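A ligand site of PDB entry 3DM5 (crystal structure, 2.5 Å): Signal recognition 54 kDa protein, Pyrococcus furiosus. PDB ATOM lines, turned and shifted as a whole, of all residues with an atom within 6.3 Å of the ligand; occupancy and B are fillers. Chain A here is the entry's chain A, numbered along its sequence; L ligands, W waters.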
ATOM      1  N   ILE A 108     -25.249   6.955  -1.320  1.00  0.00           N
ATOM      2  CA  ILE A 108     -25.385   6.648  -2.735  1.00  0.00           C
ATOM      3  C   ILE A 108     -24.023   6.535  -3.414  1.00  0.00           C
ATOM      4  O   ILE A 108     -23.011   6.914  -2.817  1.00  0.00           O
ATOM      5  CB  ILE A 108     -26.289   7.674  -3.445  1.00  0.00           C
ATOM      6  CG1 ILE A 108     -25.516   8.892  -3.902  1.00  0.00           C
ATOM      7  CG2 ILE A 108     -27.387   8.123  -2.527  1.00  0.00           C
ATOM      8  CD1 ILE A 108     -26.422  10.084  -4.018  1.00  0.00           C
ATOM      9  N   GLN A 109     -24.004   5.973  -4.614  1.00  0.00           N
ATOM     10  CA  GLN A 109     -22.759   5.825  -5.375  1.00  0.00           C
ATOM     11  C   GLN A 109     -22.042   7.174  -5.510  1.00  0.00           C
ATOM     12  O   GLN A 109     -22.660   8.206  -5.798  1.00  0.00           O
ATOM     13  CB  GLN A 109     -23.001   5.217  -6.766  1.00  0.00           C
ATOM     14  N   GLY A 110     -20.731   7.176  -5.268  1.00  0.00           N
ATOM     15  CA  GLY A 110     -19.954   8.406  -5.322  1.00  0.00           C
ATOM     16  C   GLY A 110     -20.187   9.402  -4.180  1.00  0.00           C
ATOM     17  O   GLY A 110     -19.929  10.599  -4.310  1.00  0.00           O
ATOM     18  N   SER A 111     -20.678   8.904  -3.061  1.00  0.00           N
ATOM     19  CA  SER A 111     -20.768   9.752  -1.886  1.00  0.00           C
ATOM     20  C   SER A 111     -19.443   9.693  -1.189  1.00  0.00           C
ATOM     21  O   SER A 111     -19.152  10.520  -0.346  1.00  0.00           O
ATOM     22  CB  SER A 111     -21.861   9.254  -0.943  1.00  0.00           C
ATOM     23  OG  SER A 111     -21.653   7.894  -0.587  1.00  0.00           O
ATOM     24  N   GLY A 112     -18.641   8.688  -1.527  1.00  0.00           N
ATOM     25  CA  GLY A 112     -17.409   8.430  -0.818  1.00  0.00           C
ATOM     26  C   GLY A 112     -17.627   7.511   0.385  1.00  0.00           C
ATOM     27  O   GLY A 112     -16.813   7.511   1.303  1.00  0.00           O
ATOM     28  N   LYS A 113     -18.708   6.733   0.365  1.00  0.00           N
ATOM     29  CA  LYS A 113     -19.048   5.811   1.460  1.00  0.00           C
ATOM     30  C   LYS A 113     -18.005   4.704   1.686  1.00  0.00           C
ATOM     31  O   LYS A 113     -17.490   4.545   2.801  1.00  0.00           O
ATOM     32  CB  LYS A 113     -20.396   5.158   1.212  1.00  0.00           C
ATOM     33  CG  LYS A 113     -20.845   4.246   2.314  1.00  0.00           C
ATOM     34  CD  LYS A 113     -22.167   3.606   1.972  1.00  0.00           C
ATOM     35  CE  LYS A 113     -22.001   2.326   1.149  1.00  0.00           C
ATOM     36  NZ  LYS A 113     -21.532   2.564  -0.242  1.00  0.00           N
ATOM     37  N   THR A 114     -17.695   3.930   0.648  1.00  0.00           N
ATOM     38  CA  THR A 114     -16.684   2.887   0.800  1.00  0.00           C
ATOM     39  C   THR A 114     -15.445   3.451   1.524  1.00  0.00           C
ATOM     40  O   THR A 114     -15.032   2.919   2.573  1.00  0.00           O
ATOM     41  CB  THR A 114     -16.243   2.272  -0.556  1.00  0.00           C
ATOM     42  OG1 THR A 114     -17.367   2.028  -1.402  1.00  0.00           O
ATOM     43  CG2 THR A 114     -15.521   0.982  -0.320  1.00  0.00           C
ATOM     44  N   THR A 115     -14.873   4.516   0.967  1.00  0.00           N
ATOM     45  CA  THR A 115     -13.684   5.150   1.545  1.00  0.00           C
ATOM     46  C   THR A 115     -13.918   5.587   2.986  1.00  0.00           C
ATOM     47  O   THR A 115     -13.101   5.341   3.877  1.00  0.00           O
ATOM     48  CB  THR A 115     -13.235   6.377   0.717  1.00  0.00           C
ATOM     49  OG1 THR A 115     -13.144   6.032  -0.669  1.00  0.00           O
ATOM     50  CG2 THR A 115     -11.883   6.875   1.204  1.00  0.00           C
ATOM     51  N   THR A 116     -15.038   6.273   3.221  1.00  0.00           N
ATOM     52  CA  THR A 116     -15.361   6.666   4.578  1.00  0.00           C
ATOM     53  C   THR A 116     -15.442   5.464   5.535  1.00  0.00           C
ATOM     54  O   THR A 116     -15.138   5.596   6.729  1.00  0.00           O
ATOM     55  CB  THR A 116     -16.649   7.495   4.623  1.00  0.00           C
ATOM     56  OG1 THR A 116     -16.588   8.518   3.627  1.00  0.00           O
ATOM     57  CG2 THR A 116     -16.848   8.109   6.017  1.00  0.00           C
ATOM     58  N   LYS A 119     -11.888   4.891   6.548  1.00  0.00           N
ATOM     59  CA  LYS A 119     -11.419   5.984   7.360  1.00  0.00           C
ATOM     60  C   LYS A 119     -11.887   5.864   8.798  1.00  0.00           C
ATOM     61  O   LYS A 119     -11.098   6.047   9.741  1.00  0.00           O
ATOM     62  CB  LYS A 119     -11.883   7.334   6.782  1.00  0.00           C
ATOM     63  CG  LYS A 119     -11.244   7.704   5.442  1.00  0.00           C
ATOM     64  CD  LYS A 119     -11.841   8.997   4.952  1.00  0.00           C
ATOM     65  CE  LYS A 119     -11.280   9.454   3.625  1.00  0.00           C
ATOM     66  NZ  LYS A 119     -11.707  10.873   3.401  1.00  0.00           N
ATOM     67  N   ASP A 137     -22.193  -4.644   0.530  1.00  0.00           N
ATOM     68  CA  ASP A 137     -22.466  -3.847  -0.680  1.00  0.00           C
ATOM     69  C   ASP A 137     -22.571  -4.761  -1.882  1.00  0.00           C
ATOM     70  O   ASP A 137     -21.575  -5.043  -2.554  1.00  0.00           O
ATOM     71  CB  ASP A 137     -21.362  -2.804  -0.897  1.00  0.00           C
ATOM     72  CG  ASP A 137     -21.743  -1.742  -1.952  1.00  0.00           C
ATOM     73  OD1 ASP A 137     -22.769  -1.898  -2.625  1.00  0.00           O
ATOM     74  OD2 ASP A 137     -20.981  -0.742  -2.094  1.00  0.00           O
ATOM     75  N   ARG A 140     -22.209  -2.836  -5.779  1.00  0.00           N
ATOM     76  CA  ARG A 140     -20.940  -2.780  -6.497  1.00  0.00           C
ATOM     77  C   ARG A 140     -19.918  -3.589  -5.702  1.00  0.00           C
ATOM     78  O   ARG A 140     -19.104  -3.023  -4.971  1.00  0.00           O
ATOM     79  CB  ARG A 140     -20.462  -1.343  -6.709  1.00  0.00           C
ATOM     80  CG  ARG A 140     -20.859  -0.336  -5.612  1.00  0.00           C
ATOM     81  CD  ARG A 140     -19.885   0.852  -5.587  1.00  0.00           C
ATOM     82  NE  ARG A 140     -18.514   0.372  -5.744  1.00  0.00           N
ATOM     83  CZ  ARG A 140     -17.420   0.994  -5.297  1.00  0.00           C
ATOM     84  NH1 ARG A 140     -17.513   2.145  -4.635  1.00  0.00           N
ATOM     85  NH2 ARG A 140     -16.236   0.440  -5.495  1.00  0.00           N
ATOM     86  N   GLN A 146     -11.899  -3.145  -2.729  1.00  0.00           N
ATOM     87  CA  GLN A 146     -11.485  -1.782  -2.355  1.00  0.00           C
ATOM     88  C   GLN A 146     -11.229  -1.623  -0.860  1.00  0.00           C
ATOM     89  O   GLN A 146     -10.304  -0.929  -0.444  1.00  0.00           O
ATOM     90  CB  GLN A 146     -12.522  -0.773  -2.815  1.00  0.00           C
ATOM     91  CG  GLN A 146     -12.239   0.621  -2.347  1.00  0.00           C
ATOM     92  CD  GLN A 146     -13.218   1.624  -2.926  1.00  0.00           C
ATOM     93  OE1 GLN A 146     -14.044   1.272  -3.755  1.00  0.00           O
ATOM     94  NE2 GLN A 146     -13.118   2.870  -2.478  1.00  0.00           N
ATOM     95  N   ASP A 189     -20.972  -1.735   5.817  1.00  0.00           N
ATOM     96  CA  ASP A 189     -20.982  -0.993   4.577  1.00  0.00           C
ATOM     97  C   ASP A 189     -22.091  -1.576   3.703  1.00  0.00           C
ATOM     98  O   ASP A 189     -21.915  -2.643   3.120  1.00  0.00           O
ATOM     99  CB  ASP A 189     -19.622  -1.160   3.876  1.00  0.00           C
ATOM    100  CG  ASP A 189     -19.571  -0.519   2.498  1.00  0.00           C
ATOM    101  OD1 ASP A 189     -20.126   0.589   2.335  1.00  0.00           O
ATOM    102  OD2 ASP A 189     -18.969  -1.103   1.577  1.00  0.00           O
ATOM    103  N   VAL A 246     -20.039  14.076   6.271  1.00  0.00           N
ATOM    104  CA  VAL A 246     -20.007  14.845   5.040  1.00  0.00           C
ATOM    105  C   VAL A 246     -18.626  14.738   4.419  1.00  0.00           C
ATOM    106  O   VAL A 246     -17.616  15.050   5.073  1.00  0.00           O
ATOM    107  CB  VAL A 246     -20.339  16.321   5.324  1.00  0.00           C
ATOM    108  CG1 VAL A 246     -20.258  17.133   4.061  1.00  0.00           C
ATOM    109  CG2 VAL A 246     -21.726  16.394   5.931  1.00  0.00           C
ATOM    110  N   THR A 247     -18.556  14.262   3.179  1.00  0.00           N
ATOM    111  CA  THR A 247     -17.259  14.002   2.557  1.00  0.00           C
ATOM    112  C   THR A 247     -16.856  15.097   1.572  1.00  0.00           C
ATOM    113  O   THR A 247     -17.671  15.955   1.219  1.00  0.00           O
ATOM    114  CB  THR A 247     -17.237  12.685   1.778  1.00  0.00           C
ATOM    115  OG1 THR A 247     -18.277  12.716   0.787  1.00  0.00           O
ATOM    116  CG2 THR A 247     -17.424  11.507   2.694  1.00  0.00           C
ATOM    117  N   LYS A 248     -15.591  15.046   1.134  1.00  0.00           N
ATOM    118  CA  LYS A 248     -15.100  15.867   0.039  1.00  0.00           C
ATOM    119  C   LYS A 248     -15.247  17.352   0.354  1.00  0.00           C
ATOM    120  O   LYS A 248     -15.638  18.135  -0.512  1.00  0.00           O
ATOM    121  CB  LYS A 248     -15.855  15.524  -1.244  1.00  0.00           C
ATOM    122  CG  LYS A 248     -15.758  14.064  -1.607  1.00  0.00           C
ATOM    123  CD  LYS A 248     -16.544  13.740  -2.867  1.00  0.00           C
ATOM    124  CE  LYS A 248     -16.354  12.276  -3.286  1.00  0.00           C
ATOM    125  NZ  LYS A 248     -17.207  11.891  -4.469  1.00  0.00           N
ATOM    126  N   LEU A 249     -14.981  17.736   1.602  1.00  0.00           N
ATOM    127  CA  LEU A 249     -15.008  19.150   1.949  1.00  0.00           C
ATOM    128  C   LEU A 249     -13.749  19.853   1.430  1.00  0.00           C
ATOM    129  O   LEU A 249     -13.716  21.080   1.226  1.00  0.00           O
ATOM    130  CB  LEU A 249     -15.204  19.352   3.457  1.00  0.00           C
ATOM    131  CG  LEU A 249     -16.599  19.088   4.058  1.00  0.00           C
ATOM    132  CD1 LEU A 249     -16.708  19.784   5.370  1.00  0.00           C
ATOM    133  CD2 LEU A 249     -17.706  19.552   3.161  1.00  0.00           C
ATOM    134  N   ASP A 250     -12.707  19.060   1.196  1.00  0.00           N
ATOM    135  CA  ASP A 250     -11.420  19.579   0.763  1.00  0.00           C
ATOM    136  C   ASP A 250     -11.470  20.222  -0.621  1.00  0.00           C
ATOM    137  O   ASP A 250     -11.752  19.554  -1.609  1.00  0.00           O
ATOM    138  CB  ASP A 250     -10.349  18.488   0.792  1.00  0.00           C
ATOM    139  CG  ASP A 250     -10.788  17.209   0.111  1.00  0.00           C
ATOM    140  OD1 ASP A 250     -11.906  16.731   0.397  1.00  0.00           O
ATOM    141  OD2 ASP A 250      -9.997  16.677  -0.698  1.00  0.00           O
ATOM    142  N   ILE A 272     -16.080  14.756   9.138  1.00  0.00           N
ATOM    143  CA  ILE A 272     -16.020  15.260   7.780  1.00  0.00           C
ATOM    144  C   ILE A 272     -14.902  14.543   7.089  1.00  0.00           C
ATOM    145  O   ILE A 272     -13.884  14.234   7.687  1.00  0.00           O
ATOM    146  CB  ILE A 272     -15.812  16.789   7.743  1.00  0.00           C
ATOM    147  CG1 ILE A 272     -14.628  17.209   8.608  1.00  0.00           C
ATOM    148  CG2 ILE A 272     -17.081  17.485   8.196  1.00  0.00           C
ATOM    149  CD1 ILE A 272     -14.188  18.632   8.361  1.00  0.00           C
ATOM    150  N   GLY A 273     -15.105  14.227   5.810  1.00  0.00           N
ATOM    151  CA  GLY A 273     -14.027  13.724   4.967  1.00  0.00           C
ATOM    152  C   GLY A 273     -13.267  14.857   4.294  1.00  0.00           C
ATOM    153  O   GLY A 273     -13.829  15.872   3.879  1.00  0.00           O
ATOM    154  N   THR A 274     -11.963  14.652   4.135  1.00  0.00           N
ATOM    155  CA  THR A 274     -11.008  15.731   3.939  1.00  0.00           C
ATOM    156  C   THR A 274     -10.054  15.435   2.794  1.00  0.00           C
ATOM    157  O   THR A 274      -9.187  16.235   2.454  1.00  0.00           O
ATOM    158  CB  THR A 274     -10.281  15.943   5.270  1.00  0.00           C
ATOM    159  OG1 THR A 274     -11.093  16.769   6.107  1.00  0.00           O
ATOM    160  CG2 THR A 274      -8.958  16.588   5.080  1.00  0.00           C
ATOM    161  N   GLY A 275     -10.205  14.270   2.188  1.00  0.00           N
ATOM    162  CA  GLY A 275      -9.403  13.934   1.047  1.00  0.00           C
ATOM    163  C   GLY A 275      -9.479  12.456   0.773  1.00  0.00           C
ATOM    164  O   GLY A 275     -10.225  11.740   1.412  1.00  0.00           O
ATOM    165  N   GLU A 276      -8.665  12.001  -0.174  1.00  0.00           N
ATOM    166  CA  GLU A 276      -8.779  10.643  -0.664  1.00  0.00           C
ATOM    167  C   GLU A 276      -8.093   9.579   0.194  1.00  0.00           C
ATOM    168  O   GLU A 276      -8.536   8.441   0.214  1.00  0.00           O
ATOM    169  CB  GLU A 276      -8.290  10.578  -2.115  1.00  0.00           C
ATOM    170  CG  GLU A 276      -9.082  11.482  -3.040  1.00  0.00           C
ATOM    171  CD  GLU A 276      -9.159  10.919  -4.452  1.00  0.00           C
ATOM    172  OE1 GLU A 276      -8.784   9.749  -4.630  1.00  0.00           O
ATOM    173  OE2 GLU A 276      -9.607  11.627  -5.368  1.00  0.00           O
ATOM    174  N   ASP A 280      -7.717  10.938   5.997  1.00  0.00           N
ATOM    175  CA  ASP A 280      -8.323  12.224   5.660  1.00  0.00           C
ATOM    176  C   ASP A 280      -9.742  12.350   6.183  1.00  0.00           C
ATOM    177  O   ASP A 280     -10.662  12.595   5.411  1.00  0.00           O
ATOM    178  CB  ASP A 280      -8.304  12.446   4.133  1.00  0.00           C
ATOM    179  CG  ASP A 280      -6.894  12.629   3.583  1.00  0.00           C
ATOM    180  OD1 ASP A 280      -6.009  13.104   4.328  1.00  0.00           O
ATOM    181  OD2 ASP A 280      -6.656  12.327   2.399  1.00  0.00           O
HETATM  182  P1  LIG L   1     -18.497   5.128  -3.247  1.00  0.00           P
HETATM  183  O1  LIG L   1     -18.983   6.498  -2.902  1.00  0.00           O
HETATM  184  O2  LIG L   1     -19.277   4.622  -4.434  1.00  0.00           O
HETATM  185  O3  LIG L   1     -18.686   4.221  -2.049  1.00  0.00           O
HETATM  186  O4  LIG L   1     -16.983   5.137  -3.784  1.00  0.00           O
HETATM  187  P2  LIG L   1     -15.685   5.769  -3.079  1.00  0.00           P
HETATM  188  O5  LIG L   1     -14.425   5.301  -3.748  1.00  0.00           O
HETATM  189  O6  LIG L   1     -15.635   5.478  -1.609  1.00  0.00           O
HETATM  190  O7  LIG L   1     -15.863   7.334  -3.406  1.00  0.00           O
HETATM  191  C1  LIG L   1     -15.805   7.708  -4.775  1.00  0.00           C
HETATM  192  C2  LIG L   1     -14.697   8.753  -5.006  1.00  0.00           C
HETATM  193  O8  LIG L   1     -14.719   9.849  -4.065  1.00  0.00           O
HETATM  194  C3  LIG L   1     -13.321   8.117  -4.924  1.00  0.00           C
HETATM  195  O9  LIG L   1     -12.596   8.644  -6.040  1.00  0.00           O
HETATM  196  C4  LIG L   1     -12.767   8.616  -3.602  1.00  0.00           C
HETATM  197  O10 LIG L   1     -11.379   8.819  -3.636  1.00  0.00           O
HETATM  198  C5  LIG L   1     -13.415   9.969  -3.468  1.00  0.00           C
HETATM  199  N1  LIG L   1     -13.542  10.451  -2.087  1.00  0.00           N
HETATM  200  C6  LIG L   1     -14.188   9.892  -1.050  1.00  0.00           C
HETATM  201  N2  LIG L   1     -14.103  10.683   0.049  1.00  0.00           N
HETATM  202  C7  LIG L   1     -13.401  11.783  -0.296  1.00  0.00           C
HETATM  203  C8  LIG L   1     -12.934  13.041   0.353  1.00  0.00           C
HETATM  204  O11 LIG L   1     -13.186  13.306   1.550  1.00  0.00           O
HETATM  205  N3  LIG L   1     -12.220  13.888  -0.395  1.00  0.00           N
HETATM  206  C9  LIG L   1     -11.929  13.664  -1.686  1.00  0.00           C
HETATM  207  N4  LIG L   1     -11.218  14.583  -2.366  1.00  0.00           N
HETATM  208  N5  LIG L   1     -12.333  12.561  -2.347  1.00  0.00           N
HETATM  209  C10 LIG L   1     -13.046  11.620  -1.709  1.00  0.00           C
HETATM  210  O   HOH W   1     -14.187  10.283   2.733  1.00  0.00           O
HETATM  211  O   HOH W   2     -18.174   5.238  -6.780  1.00  0.00           O
HETATM  212  O   HOH W   3     -12.829  12.847  -5.470  1.00  0.00           O
HETATM  213  O   HOH W   4     -21.479   3.428  -2.641  1.00  0.00           O
HETATM  214  O   HOH W   5     -14.929   4.500  -6.240  1.00  0.00           O
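The backbone carbonyl oxygen of Ser 111 lies within hydrogen-bond range of the side-chain hydroxyl of Thr 247 (2.6 Å).
N of Glu 276 sits at hydrogen-bond distance from OD2 of Asp 280.
The backbone carbonyl oxygen (O) of Gly 112 sits at hydrogen-bond distance from the side-chain hydroxyl (OG1) of Thr 116 (2.5 Å).
The backbone NH of Lys 113 is in hydrogen-bond range of the side-chain hydroxyl of Ser 111.
The guanidinium group (NH2) of Arg 140 is in hydrogen-bond range of the side-chain amide oxygen (OE1) of Gln 146, at 2.9 Å.
NZ of Lys 248 sits at hydrogen-bond distance from O of Gly 110 (3.0 Å).
The backbone carbonyl oxygen of Ile 108 is in hydrogen-bond range of the side-chain hydroxyl of Ser 111 (2.8 Å).
OD1 of Asp 189 is in salt-bridge range of NZ of Lys 113 (3.5 Å).
Residues that only touch the ligand: Gly 273 (3.2 Å) and Gln 109 (3.8 Å).
Within 4 Å of the ligand: Gln 109, Gly 110, Ser 111, Gly 112, Lys 113, Thr 114, Thr 115, Lys 119, Arg 140, Gln 146, Lys 248, Asp 250, Gly 273, Thr 274, Gly 275 and Glu 276.
Along chain A the residues within 4 Å of the ligand span positions 109 to 276.
Water W1 lies within hydrogen-bond range of the side-chain amino group (NZ) of Lys 119 (2.6 Å), a nitrogen (N2) of the ligand (2.7 Å) and the side-chain hydroxyl (OG1) of Thr 116 (3.1 Å).
Water W4 lies within hydrogen-bond range of the side-chain amino group (NZ) of Lys 113 (2.6 Å) and an oxygen (O3) of the ligand (3.0 Å).
Water W3 lies within hydrogen-bond range of N5 of the ligand (3.2 Å) and OE2 of Glu 276 (3.4 Å).
O1 of the ligand is in hydrogen-bond range of N of Gly 112, 2.6 Å away.
The backbone NH (N) of Thr 274 is in hydrogen-bond range of an oxygen (O11) of the ligand (3.2 Å).
O1 of the ligand is in hydrogen-bond range of N of Lys 113 (3.3 Å).
N of Thr 114 lies within hydrogen-bond range of O3 of the ligand (2.9 Å).
OG1 of Thr 115 lies within hydrogen-bond range of O6 of the ligand, at 2.7 Å.
O of Gly 275 lies close to N3 of the ligand (3.4 Å).
O2 of the ligand is in salt-bridge range of NH1 of Arg 140, 3.0 Å away.
O3 of the ligand is in hydrogen-bond range of OG1 of Thr 114, at 2.6 Å.
An oxygen (O5) of the ligand sits at hydrogen-bond distance from the side-chain amide nitrogen (NE2) of Gln 146, at 3.0 Å.
The side-chain amino group (NZ) of Lys 113 is in salt-bridge range of an oxygen (O3) of the ligand, at 3.8 Å.
The side-chain carboxylate of Asp 250 lies within hydrogen-bond range of a nitrogen (N4) of the ligand, 2.9 Å away.
O10 of the ligand lies within hydrogen-bond range of OE1 of Glu 276.
An oxygen (O11) of the ligand sits at hydrogen-bond distance from the backbone NH (N) of Gly 275 (3.2 Å).
NZ of Lys 248 sits close to O8 of the ligand.
An oxygen (O1) of the ligand is in hydrogen-bond range of the backbone NH (N) of Ser 111 (2.9 Å).
The backbone NH of Thr 115 sits at hydrogen-bond distance from an oxygen (O6) of the ligand (2.9 Å).
An oxygen (O11) of the ligand is in hydrogen-bond range of the backbone NH (N) of Lys 248, at 3.0 Å.
The side-chain amino group of Lys 119 sits at hydrogen-bond distance from an oxygen (O11) of the ligand, 3.4 Å away.
The backbone NH (N) of Gly 110 lies within hydrogen-bond range of an oxygen (O1) of the ligand (3.0 Å).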
